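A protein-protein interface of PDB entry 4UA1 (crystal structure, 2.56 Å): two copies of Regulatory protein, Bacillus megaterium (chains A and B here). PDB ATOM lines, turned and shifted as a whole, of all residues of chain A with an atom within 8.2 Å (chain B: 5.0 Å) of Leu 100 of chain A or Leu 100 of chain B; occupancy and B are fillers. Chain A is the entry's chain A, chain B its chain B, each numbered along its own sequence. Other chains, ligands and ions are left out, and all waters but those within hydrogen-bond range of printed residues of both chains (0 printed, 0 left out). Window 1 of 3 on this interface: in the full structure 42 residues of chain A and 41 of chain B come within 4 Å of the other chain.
OE1 of Glu 104 of chain B sits at hydrogen-bond distance from NE2 of Gln 94 of chain A (2.8 Å).
The side-chain carboxylate (OE2) of Glu 98 of chain A lies close to the side-chain amide oxygen (OE1) of Gln 94 of chain A.
Leu 58 of chain A touches Ile 103 of chain B.
CG of Glu 104 of chain B touches CG2 of Ile 90 of chain A, at 3.8 Å.
Ile 93 of chain A touches Leu 100 of chain B.
Leu 100 of chain B touches Ile 97 of chain A (CB to CG1, 3.5 Å).
Glu 104 of chain B touches Ile 97 of chain A (OE2 to CD1, 3.4 Å).
CG2 of Ile 93 of chain B touches O of Leu 100 of chain A, at 3.6 Å.
CG1 of Ile 97 of chain B touches CB of Leu 100 of chain A, at 3.7 Å.
Leu 100 of chain A touches Leu 100 of chain B.
Ile 97 of chain B touches Lys 101 of chain A.
Ile 97 of chain B touches Glu 104 of chain A.
Of the printed residues of chain B, Ile 93 of chain A touches Leu 100.
Of the printed residues of chain B, Gln 94 of chain A touches Glu 104 (2.8 Å).
Of the printed residues of chain B, Leu 100 of chain A touches Ile 93, Ile 97 and Leu 100.
Ile 103 of chain A touches none of the printed residues of chain B.
Of the printed residues of chain B, Leu 107 of chain A touches Ile 93 (3.98 Å).
Printed residues of chain A within 4 Å of Ile 93 of chain B: Leu 100 and Leu 107.
Lys 96 of chain B touches none of the printed residues of chain A.
Printed residues of chain A within 4 Å of Ile 97 of chain B: Leu 100 (3.7 Å), Lys 101 (3.9 Å) and Glu 104 (3.4 Å).
Of chain A, only Ile 93, Ile 97 and Leu 100 come within 4 Å of Leu 100 of chain B.
The nearest printed residue of chain A that does not touch Ile 93 of chain B is Glu 104 of chain A (4.1 Å).
Among the printed residues, no Asp or Glu carboxylate lies within 4 Å of a Lys or Arg side-chain nitrogen of the other chain.
Ile 97 of chain A touches Leu 100 of chain B, and with the chains exchanged Leu 100 of chain A touches Ile 97 of chain B.
Ile 97 of chain A touches Lys 101 of chain B, and with the chains exchanged Lys 101 of chain A touches Ile 97 of chain B.
Ile 97 of chain A touches Glu 104 of chain B, and with the chains exchanged Glu 104 of chain A touches Ile 97 of chain B.
Leu 100 of chain A touches its own counterpart, Leu 100 of chain B.
Positions printed for both chains: 93, 96, 97, 98, 99, 100, 101, 102, 103 and 104.
Of the 14 pairs that touch across the chains among the printed residues, 9 have their exchanged pair printed and touching as well.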
ATOM      1  N   GLU A  57      16.942 -33.486 -16.152  1.00  0.00           N
ATOM      2  CA  GLU A  57      15.766 -33.695 -16.982  1.00  0.00           C
ATOM      3  C   GLU A  57      14.584 -34.102 -16.104  1.00  0.00           C
ATOM      4  O   GLU A  57      13.434 -33.985 -16.508  1.00  0.00           O
ATOM      5  CB  GLU A  57      16.051 -34.741 -18.054  1.00  0.00           C
ATOM      6  CG  GLU A  57      17.168 -34.320 -18.996  1.00  0.00           C
ATOM      7  CD  GLU A  57      17.576 -35.412 -19.965  1.00  0.00           C
ATOM      8  OE1 GLU A  57      17.370 -36.606 -19.645  1.00  0.00           O
ATOM      9  OE2 GLU A  57      18.113 -35.067 -21.042  1.00  0.00           O
ATOM     10  N   LEU A  58      14.879 -34.556 -14.889  1.00  0.00           N
ATOM     11  CA  LEU A  58      13.851 -34.926 -13.932  1.00  0.00           C
ATOM     12  C   LEU A  58      13.500 -33.823 -12.923  1.00  0.00           C
ATOM     13  O   LEU A  58      12.744 -34.053 -11.981  1.00  0.00           O
ATOM     14  CB  LEU A  58      14.282 -36.189 -13.203  1.00  0.00           C
ATOM     15  CG  LEU A  58      14.241 -37.352 -14.193  1.00  0.00           C
ATOM     16  CD1 LEU A  58      14.808 -38.625 -13.577  1.00  0.00           C
ATOM     17  CD2 LEU A  58      12.828 -37.550 -14.705  1.00  0.00           C
ATOM     18  N   GLY A  59      14.073 -32.640 -13.085  1.00  0.00           N
ATOM     19  CA  GLY A  59      13.706 -31.528 -12.234  1.00  0.00           C
ATOM     20  C   GLY A  59      14.603 -31.270 -11.033  1.00  0.00           C
ATOM     21  O   GLY A  59      14.274 -30.434 -10.189  1.00  0.00           O
ATOM     22  N   ILE A  90       9.996 -35.816  -5.901  1.00  0.00           N
ATOM     23  CA  ILE A  90       8.600 -36.050  -6.237  1.00  0.00           C
ATOM     24  C   ILE A  90       7.690 -35.058  -5.511  1.00  0.00           C
ATOM     25  O   ILE A  90       6.790 -34.459  -6.109  1.00  0.00           O
ATOM     26  CB  ILE A  90       8.176 -37.471  -5.867  1.00  0.00           C
ATOM     27  CG1 ILE A  90       8.968 -38.508  -6.679  1.00  0.00           C
ATOM     28  CG2 ILE A  90       6.649 -37.640  -6.021  1.00  0.00           C
ATOM     29  CD1 ILE A  90       8.829 -39.956  -6.144  1.00  0.00           C
ATOM     30  N   ASP A  92       8.505 -32.164  -4.388  1.00  0.00           N
ATOM     31  CA  ASP A  92       8.785 -30.825  -4.898  1.00  0.00           C
ATOM     32  C   ASP A  92       8.013 -30.570  -6.205  1.00  0.00           C
ATOM     33  O   ASP A  92       7.386 -29.505  -6.403  1.00  0.00           O
ATOM     34  CB  ASP A  92      10.280 -30.654  -5.066  1.00  0.00           C
ATOM     35  CG  ASP A  92      10.675 -29.233  -5.385  1.00  0.00           C
ATOM     36  OD1 ASP A  92      10.244 -28.314  -4.652  1.00  0.00           O
ATOM     37  OD2 ASP A  92      11.449 -29.036  -6.349  1.00  0.00           O
ATOM     38  N   ILE A  93       8.039 -31.574  -7.077  1.00  0.00           N
ATOM     39  CA  ILE A  93       7.271 -31.576  -8.309  1.00  0.00           C
ATOM     40  C   ILE A  93       5.776 -31.410  -8.018  1.00  0.00           C
ATOM     41  O   ILE A  93       5.070 -30.676  -8.728  1.00  0.00           O
ATOM     42  CB  ILE A  93       7.502 -32.874  -9.099  1.00  0.00           C
ATOM     43  CG1 ILE A  93       8.979 -33.001  -9.454  1.00  0.00           C
ATOM     44  CG2 ILE A  93       6.681 -32.880 -10.384  1.00  0.00           C
ATOM     45  CD1 ILE A  93       9.478 -31.857 -10.284  1.00  0.00           C
ATOM     46  N   GLN A  94       5.310 -32.065  -6.954  1.00  0.00           N
ATOM     47  CA  GLN A  94       3.903 -31.985  -6.553  1.00  0.00           C
ATOM     48  C   GLN A  94       3.518 -30.557  -6.144  1.00  0.00           C
ATOM     49  O   GLN A  94       2.470 -30.050  -6.598  1.00  0.00           O
ATOM     50  CB  GLN A  94       3.628 -32.960  -5.415  1.00  0.00           C
ATOM     51  CG  GLN A  94       2.173 -33.108  -4.944  1.00  0.00           C
ATOM     52  CD  GLN A  94       1.119 -33.297  -6.049  1.00  0.00           C
ATOM     53  OE1 GLN A  94      -0.016 -32.821  -5.907  1.00  0.00           O
ATOM     54  NE2 GLN A  94       1.477 -34.000  -7.132  1.00  0.00           N
ATOM     55  N   ARG A  95       4.371 -29.900  -5.342  1.00  0.00           N
ATOM     56  CA  ARG A  95       4.151 -28.483  -5.025  1.00  0.00           C
ATOM     57  C   ARG A  95       4.023 -27.638  -6.287  1.00  0.00           C
ATOM     58  O   ARG A  95       3.068 -26.852  -6.427  1.00  0.00           O
ATOM     59  CB  ARG A  95       5.284 -27.899  -4.174  1.00  0.00           C
ATOM     60  CG  ARG A  95       5.333 -28.451  -2.789  1.00  0.00           C
ATOM     61  CD  ARG A  95       6.316 -27.700  -1.928  1.00  0.00           C
ATOM     62  NE  ARG A  95       6.360 -28.250  -0.576  1.00  0.00           N
ATOM     63  CZ  ARG A  95       5.506 -27.936   0.398  1.00  0.00           C
ATOM     64  NH1 ARG A  95       4.506 -27.081   0.185  1.00  0.00           N
ATOM     65  NH2 ARG A  95       5.652 -28.490   1.590  1.00  0.00           N
ATOM     66  N   LYS A  96       4.956 -27.826  -7.220  1.00  0.00           N
ATOM     67  CA  LYS A  96       4.923 -27.016  -8.434  1.00  0.00           C
ATOM     68  C   LYS A  96       3.595 -27.214  -9.182  1.00  0.00           C
ATOM     69  O   LYS A  96       2.932 -26.233  -9.584  1.00  0.00           O
ATOM     70  CB  LYS A  96       6.118 -27.345  -9.337  1.00  0.00           C
ATOM     71  CG  LYS A  96       7.473 -26.977  -8.740  1.00  0.00           C
ATOM     72  CD  LYS A  96       8.610 -27.216  -9.752  1.00  0.00           C
ATOM     73  CE  LYS A  96      10.008 -27.171  -9.110  1.00  0.00           C
ATOM     74  NZ  LYS A  96      10.213 -26.011  -8.194  1.00  0.00           N
ATOM     75  N   ILE A  97       3.187 -28.475  -9.320  1.00  0.00           N
ATOM     76  CA  ILE A  97       1.912 -28.804  -9.952  1.00  0.00           C
ATOM     77  C   ILE A  97       0.750 -28.077  -9.286  1.00  0.00           C
ATOM     78  O   ILE A  97      -0.140 -27.555  -9.970  1.00  0.00           O
ATOM     79  CB  ILE A  97       1.669 -30.318  -9.943  1.00  0.00           C
ATOM     80  CG1 ILE A  97       2.528 -30.955 -11.033  1.00  0.00           C
ATOM     81  CG2 ILE A  97       0.201 -30.670 -10.211  1.00  0.00           C
ATOM     82  CD1 ILE A  97       2.427 -32.456 -11.121  1.00  0.00           C
ATOM     83  N   GLU A  98       0.758 -28.035  -7.956  1.00  0.00           N
ATOM     84  CA  GLU A  98      -0.322 -27.365  -7.252  1.00  0.00           C
ATOM     85  C   GLU A  98      -0.303 -25.841  -7.501  1.00  0.00           C
ATOM     86  O   GLU A  98      -1.364 -25.212  -7.641  1.00  0.00           O
ATOM     87  CB  GLU A  98      -0.252 -27.713  -5.762  1.00  0.00           C
ATOM     88  CG  GLU A  98      -0.401 -29.230  -5.517  1.00  0.00           C
ATOM     89  CD  GLU A  98      -0.032 -29.688  -4.105  1.00  0.00           C
ATOM     90  OE1 GLU A  98       0.644 -28.929  -3.362  1.00  0.00           O
ATOM     91  OE2 GLU A  98      -0.417 -30.827  -3.745  1.00  0.00           O
ATOM     92  N   ASP A  99       0.898 -25.260  -7.576  1.00  0.00           N
ATOM     93  CA  ASP A  99       1.044 -23.837  -7.874  1.00  0.00           C
ATOM     94  C   ASP A  99       0.457 -23.506  -9.257  1.00  0.00           C
ATOM     95  O   ASP A  99      -0.310 -22.531  -9.453  1.00  0.00           O
ATOM     96  CB  ASP A  99       2.516 -23.431  -7.795  1.00  0.00           C
ATOM     97  CG  ASP A  99       3.053 -23.454  -6.356  1.00  0.00           C
ATOM     98  OD1 ASP A  99       2.235 -23.550  -5.407  1.00  0.00           O
ATOM     99  OD2 ASP A  99       4.294 -23.369  -6.162  1.00  0.00           O
ATOM    100  N   LEU A 100       0.766 -24.383 -10.202  1.00  0.00           N
ATOM    101  CA  LEU A 100       0.215 -24.286 -11.538  1.00  0.00           C
ATOM    102  C   LEU A 100      -1.330 -24.418 -11.559  1.00  0.00           C
ATOM    103  O   LEU A 100      -2.019 -23.703 -12.298  1.00  0.00           O
ATOM    104  CB  LEU A 100       0.895 -25.339 -12.416  1.00  0.00           C
ATOM    105  CG  LEU A 100       2.336 -24.908 -12.726  1.00  0.00           C
ATOM    106  CD1 LEU A 100       3.053 -25.948 -13.533  1.00  0.00           C
ATOM    107  CD2 LEU A 100       2.309 -23.599 -13.493  1.00  0.00           C
ATOM    108  N   LYS A 101      -1.880 -25.290 -10.734  1.00  0.00           N
ATOM    109  CA  LYS A 101      -3.333 -25.399 -10.647  1.00  0.00           C
ATOM    110  C   LYS A 101      -3.946 -24.130 -10.050  1.00  0.00           C
ATOM    111  O   LYS A 101      -5.048 -23.706 -10.462  1.00  0.00           O
ATOM    112  CB  LYS A 101      -3.737 -26.634  -9.853  1.00  0.00           C
ATOM    113  CG  LYS A 101      -3.711 -27.899 -10.694  1.00  0.00           C
ATOM    114  CD  LYS A 101      -4.030 -29.115  -9.870  1.00  0.00           C
ATOM    115  CE  LYS A 101      -4.407 -30.258 -10.763  1.00  0.00           C
ATOM    116  NZ  LYS A 101      -5.715 -29.934 -11.406  1.00  0.00           N
ATOM    117  N   ARG A 102      -3.249 -23.512  -9.091  1.00  0.00           N
ATOM    118  CA  ARG A 102      -3.772 -22.244  -8.582  1.00  0.00           C
ATOM    119  C   ARG A 102      -3.826 -21.197  -9.683  1.00  0.00           C
ATOM    120  O   ARG A 102      -4.844 -20.512  -9.840  1.00  0.00           O
ATOM    121  CB  ARG A 102      -2.970 -21.715  -7.391  1.00  0.00           C
ATOM    122  CG  ARG A 102      -3.396 -22.364  -6.083  1.00  0.00           C
ATOM    123  CD  ARG A 102      -2.560 -21.893  -4.898  1.00  0.00           C
ATOM    124  NE  ARG A 102      -1.280 -22.576  -4.845  1.00  0.00           N
ATOM    125  CZ  ARG A 102      -1.099 -23.787  -4.337  1.00  0.00           C
ATOM    126  NH1 ARG A 102      -2.112 -24.455  -3.814  1.00  0.00           N
ATOM    127  NH2 ARG A 102       0.111 -24.325  -4.349  1.00  0.00           N
ATOM    128  N   ILE A 103      -2.775 -21.132 -10.496  1.00  0.00           N
ATOM    129  CA  ILE A 103      -2.750 -20.141 -11.577  1.00  0.00           C
ATOM    130  C   ILE A 103      -3.860 -20.410 -12.612  1.00  0.00           C
ATOM    131  O   ILE A 103      -4.618 -19.501 -13.021  1.00  0.00           O
ATOM    132  CB  ILE A 103      -1.388 -20.122 -12.267  1.00  0.00           C
ATOM    133  CG1 ILE A 103      -0.320 -19.550 -11.329  1.00  0.00           C
ATOM    134  CG2 ILE A 103      -1.462 -19.354 -13.565  1.00  0.00           C
ATOM    135  CD1 ILE A 103       1.085 -19.825 -11.804  1.00  0.00           C
ATOM    136  N   GLU A 104      -3.994 -21.674 -12.979  1.00  0.00           N
ATOM    137  CA  GLU A 104      -5.047 -22.081 -13.893  1.00  0.00           C
ATOM    138  C   GLU A 104      -6.431 -21.656 -13.427  1.00  0.00           C
ATOM    139  O   GLU A 104      -7.223 -21.114 -14.211  1.00  0.00           O
ATOM    140  CB  GLU A 104      -5.027 -23.585 -14.072  1.00  0.00           C
ATOM    141  CG  GLU A 104      -5.512 -24.011 -15.416  1.00  0.00           C
ATOM    142  CD  GLU A 104      -5.552 -25.509 -15.548  1.00  0.00           C
ATOM    143  OE1 GLU A 104      -5.106 -26.204 -14.608  1.00  0.00           O
ATOM    144  OE2 GLU A 104      -6.028 -25.989 -16.594  1.00  0.00           O
ATOM    145  N   ARG A 105      -6.743 -21.922 -12.165  1.00  0.00           N
ATOM    146  CA  ARG A 105      -8.058 -21.539 -11.642  1.00  0.00           C
ATOM    147  C   ARG A 105      -8.235 -19.997 -11.629  1.00  0.00           C
ATOM    148  O   ARG A 105      -9.296 -19.484 -11.953  1.00  0.00           O
ATOM    149  CB  ARG A 105      -8.270 -22.153 -10.252  1.00  0.00           C
ATOM    150  CG  ARG A 105      -8.495 -23.682 -10.282  1.00  0.00           C
ATOM    151  CD  ARG A 105      -8.932 -24.232  -8.924  1.00  0.00           C
ATOM    152  NE  ARG A 105      -7.905 -23.984  -7.921  1.00  0.00           N
ATOM    153  CZ  ARG A 105      -6.955 -24.849  -7.568  1.00  0.00           C
ATOM    154  NH1 ARG A 105      -6.897 -26.060  -8.108  1.00  0.00           N
ATOM    155  NH2 ARG A 105      -6.074 -24.506  -6.636  1.00  0.00           N
ATOM    156  N   MET A 106      -7.163 -19.280 -11.296  1.00  0.00           N
ATOM    157  CA  MET A 106      -7.149 -17.834 -11.379  1.00  0.00           C
ATOM    158  C   MET A 106      -7.582 -17.363 -12.792  1.00  0.00           C
ATOM    159  O   MET A 106      -8.441 -16.474 -12.945  1.00  0.00           O
ATOM    160  CB  MET A 106      -5.745 -17.335 -11.043  1.00  0.00           C
ATOM    161  CG  MET A 106      -5.701 -16.027 -10.276  1.00  0.00           C
ATOM    162  SD  MET A 106      -4.069 -15.588  -9.589  1.00  0.00           S
ATOM    163  CE  MET A 106      -3.617 -17.055  -8.668  1.00  0.00           C
ATOM    164  N   LEU A 107      -7.013 -17.993 -13.815  1.00  0.00           N
ATOM    165  CA  LEU A 107      -7.346 -17.691 -15.196  1.00  0.00           C
ATOM    166  C   LEU A 107      -8.804 -18.063 -15.526  1.00  0.00           C
ATOM    167  O   LEU A 107      -9.507 -17.317 -16.223  1.00  0.00           O
ATOM    168  CB  LEU A 107      -6.391 -18.438 -16.122  1.00  0.00           C
ATOM    169  CG  LEU A 107      -4.907 -18.068 -16.074  1.00  0.00           C
ATOM    170  CD1 LEU A 107      -4.121 -19.164 -16.777  1.00  0.00           C
ATOM    171  CD2 LEU A 107      -4.684 -16.736 -16.748  1.00  0.00           C
ATOM    172  N   ILE B  93      -1.118 -23.895 -19.596  1.00  0.00           N
ATOM    173  CA  ILE B  93      -0.838 -24.295 -18.231  1.00  0.00           C
ATOM    174  C   ILE B  93      -1.176 -25.762 -18.050  1.00  0.00           C
ATOM    175  O   ILE B  93      -0.476 -26.482 -17.329  1.00  0.00           O
ATOM    176  CB  ILE B  93      -1.626 -23.458 -17.200  1.00  0.00           C
ATOM    177  CG1 ILE B  93      -1.349 -21.958 -17.380  1.00  0.00           C
ATOM    178  CG2 ILE B  93      -1.284 -23.910 -15.783  1.00  0.00           C
ATOM    179  CD1 ILE B  93       0.077 -21.586 -17.214  1.00  0.00           C
ATOM    180  N   LYS B  96       1.677 -27.822 -19.318  1.00  0.00           N
ATOM    181  CA  LYS B  96       2.827 -27.799 -18.388  1.00  0.00           C
ATOM    182  C   LYS B  96       2.606 -28.746 -17.222  1.00  0.00           C
ATOM    183  O   LYS B  96       3.508 -29.489 -16.786  1.00  0.00           O
ATOM    184  CB  LYS B  96       3.077 -26.408 -17.816  1.00  0.00           C
ATOM    185  CG  LYS B  96       3.538 -25.351 -18.804  1.00  0.00           C
ATOM    186  CD  LYS B  96       3.875 -24.046 -18.067  1.00  0.00           C
ATOM    187  CE  LYS B  96       4.035 -22.876 -19.018  1.00  0.00           C
ATOM    188  NZ  LYS B  96       4.889 -23.225 -20.201  1.00  0.00           N
ATOM    189  N   ILE B  97       1.392 -28.681 -16.697  1.00  0.00           N
ATOM    190  CA  ILE B  97       0.995 -29.556 -15.612  1.00  0.00           C
ATOM    191  C   ILE B  97       1.183 -31.026 -15.988  1.00  0.00           C
ATOM    192  O   ILE B  97       1.730 -31.825 -15.204  1.00  0.00           O
ATOM    193  CB  ILE B  97      -0.471 -29.309 -15.216  1.00  0.00           C
ATOM    194  CG1 ILE B  97      -0.616 -27.935 -14.551  1.00  0.00           C
ATOM    195  CG2 ILE B  97      -0.959 -30.418 -14.307  1.00  0.00           C
ATOM    196  CD1 ILE B  97      -2.047 -27.560 -14.184  1.00  0.00           C
ATOM    197  N   GLU B  98       0.764 -31.374 -17.206  1.00  0.00           N
ATOM    198  CA  GLU B  98       0.805 -32.765 -17.623  1.00  0.00           C
ATOM    199  C   GLU B  98       2.255 -33.204 -17.734  1.00  0.00           C
ATOM    200  O   GLU B  98       2.618 -34.313 -17.333  1.00  0.00           O
ATOM    201  CB  GLU B  98       0.073 -32.969 -18.953  1.00  0.00           C
ATOM    202  CG  GLU B  98      -1.421 -32.536 -18.986  1.00  0.00           C
ATOM    203  CD  GLU B  98      -2.356 -33.329 -18.080  1.00  0.00           C
ATOM    204  OE1 GLU B  98      -2.054 -33.553 -16.883  1.00  0.00           O
ATOM    205  OE2 GLU B  98      -3.432 -33.720 -18.578  1.00  0.00           O
ATOM    206  N   ASP B  99       3.098 -32.307 -18.236  1.00  0.00           N
ATOM    207  CA  ASP B  99       4.522 -32.615 -18.356  1.00  0.00           C
ATOM    208  C   ASP B  99       5.177 -32.928 -16.996  1.00  0.00           C
ATOM    209  O   ASP B  99       5.975 -33.890 -16.867  1.00  0.00           O
ATOM    210  CB  ASP B  99       5.222 -31.458 -19.028  1.00  0.00           C
ATOM    211  CG  ASP B  99       4.855 -31.334 -20.493  1.00  0.00           C
ATOM    212  OD1 ASP B  99       4.254 -32.282 -21.056  1.00  0.00           O
ATOM    213  OD2 ASP B  99       5.184 -30.286 -21.091  1.00  0.00           O
ATOM    214  N   LEU B 100       4.823 -32.121 -15.993  1.00  0.00           N
ATOM    215  CA  LEU B 100       5.260 -32.356 -14.615  1.00  0.00           C
ATOM    216  C   LEU B 100       4.739 -33.667 -14.037  1.00  0.00           C
ATOM    217  O   LEU B 100       5.428 -34.352 -13.273  1.00  0.00           O
ATOM    218  CB  LEU B 100       4.818 -31.210 -13.706  1.00  0.00           C
ATOM    219  CG  LEU B 100       5.616 -29.937 -13.920  1.00  0.00           C
ATOM    220  CD1 LEU B 100       5.126 -28.832 -12.983  1.00  0.00           C
ATOM    221  CD2 LEU B 100       7.093 -30.223 -13.741  1.00  0.00           C
ATOM    222  N   LYS B 101       3.507 -34.006 -14.387  1.00  0.00           N
ATOM    223  CA  LYS B 101       2.956 -35.282 -13.974  1.00  0.00           C
ATOM    224  C   LYS B 101       3.720 -36.453 -14.601  1.00  0.00           C
ATOM    225  O   LYS B 101       3.946 -37.489 -13.976  1.00  0.00           O
ATOM    226  CB  LYS B 101       1.488 -35.357 -14.362  1.00  0.00           C
ATOM    227  CG  LYS B 101       0.552 -34.647 -13.402  1.00  0.00           C
ATOM    228  CD  LYS B 101      -0.872 -34.722 -13.906  1.00  0.00           C
ATOM    229  CE  LYS B 101      -1.862 -34.389 -12.820  1.00  0.00           C
ATOM    230  NZ  LYS B 101      -1.465 -33.156 -12.096  1.00  0.00           N
ATOM    231  N   ARG B 102       4.120 -36.287 -15.849  1.00  0.00           N
ATOM    232  CA  ARG B 102       4.872 -37.325 -16.522  1.00  0.00           C
ATOM    233  C   ARG B 102       6.218 -37.527 -15.811  1.00  0.00           C
ATOM    234  O   ARG B 102       6.676 -38.659 -15.622  1.00  0.00           O
ATOM    235  CB  ARG B 102       5.007 -36.957 -17.986  1.00  0.00           C
ATOM    236  CG  ARG B 102       3.696 -37.237 -18.722  1.00  0.00           C
ATOM    237  CD  ARG B 102       3.728 -36.766 -20.150  1.00  0.00           C
ATOM    238  NE  ARG B 102       4.692 -37.514 -20.936  1.00  0.00           N
ATOM    239  CZ  ARG B 102       5.289 -37.033 -22.014  1.00  0.00           C
ATOM    240  NH1 ARG B 102       5.014 -35.803 -22.419  1.00  0.00           N
ATOM    241  NH2 ARG B 102       6.158 -37.779 -22.675  1.00  0.00           N
ATOM    242  N   ILE B 103       6.840 -36.422 -15.405  1.00  0.00           N
ATOM    243  CA  ILE B 103       8.082 -36.516 -14.644  1.00  0.00           C
ATOM    244  C   ILE B 103       7.880 -37.177 -13.277  1.00  0.00           C
ATOM    245  O   ILE B 103       8.656 -38.025 -12.848  1.00  0.00           O
ATOM    246  CB  ILE B 103       8.696 -35.141 -14.459  1.00  0.00           C
ATOM    247  CG1 ILE B 103       9.346 -34.726 -15.765  1.00  0.00           C
ATOM    248  CG2 ILE B 103       9.727 -35.139 -13.333  1.00  0.00           C
ATOM    249  CD1 ILE B 103       9.625 -33.239 -15.845  1.00  0.00           C
ATOM    250  N   GLU B 104       6.826 -36.781 -12.598  1.00  0.00           N
ATOM    251  CA  GLU B 104       6.494 -37.374 -11.331  1.00  0.00           C
ATOM    252  C   GLU B 104       6.370 -38.894 -11.474  1.00  0.00           C
ATOM    253  O   GLU B 104       6.952 -39.648 -10.704  1.00  0.00           O
ATOM    254  CB  GLU B 104       5.211 -36.757 -10.829  1.00  0.00           C
ATOM    255  CG  GLU B 104       5.081 -36.648  -9.332  1.00  0.00           C
ATOM    256  CD  GLU B 104       3.734 -36.039  -8.982  1.00  0.00           C
ATOM    257  OE1 GLU B 104       3.342 -36.001  -7.792  1.00  0.00           O
ATOM    258  OE2 GLU B 104       3.051 -35.623  -9.940  1.00  0.00           O
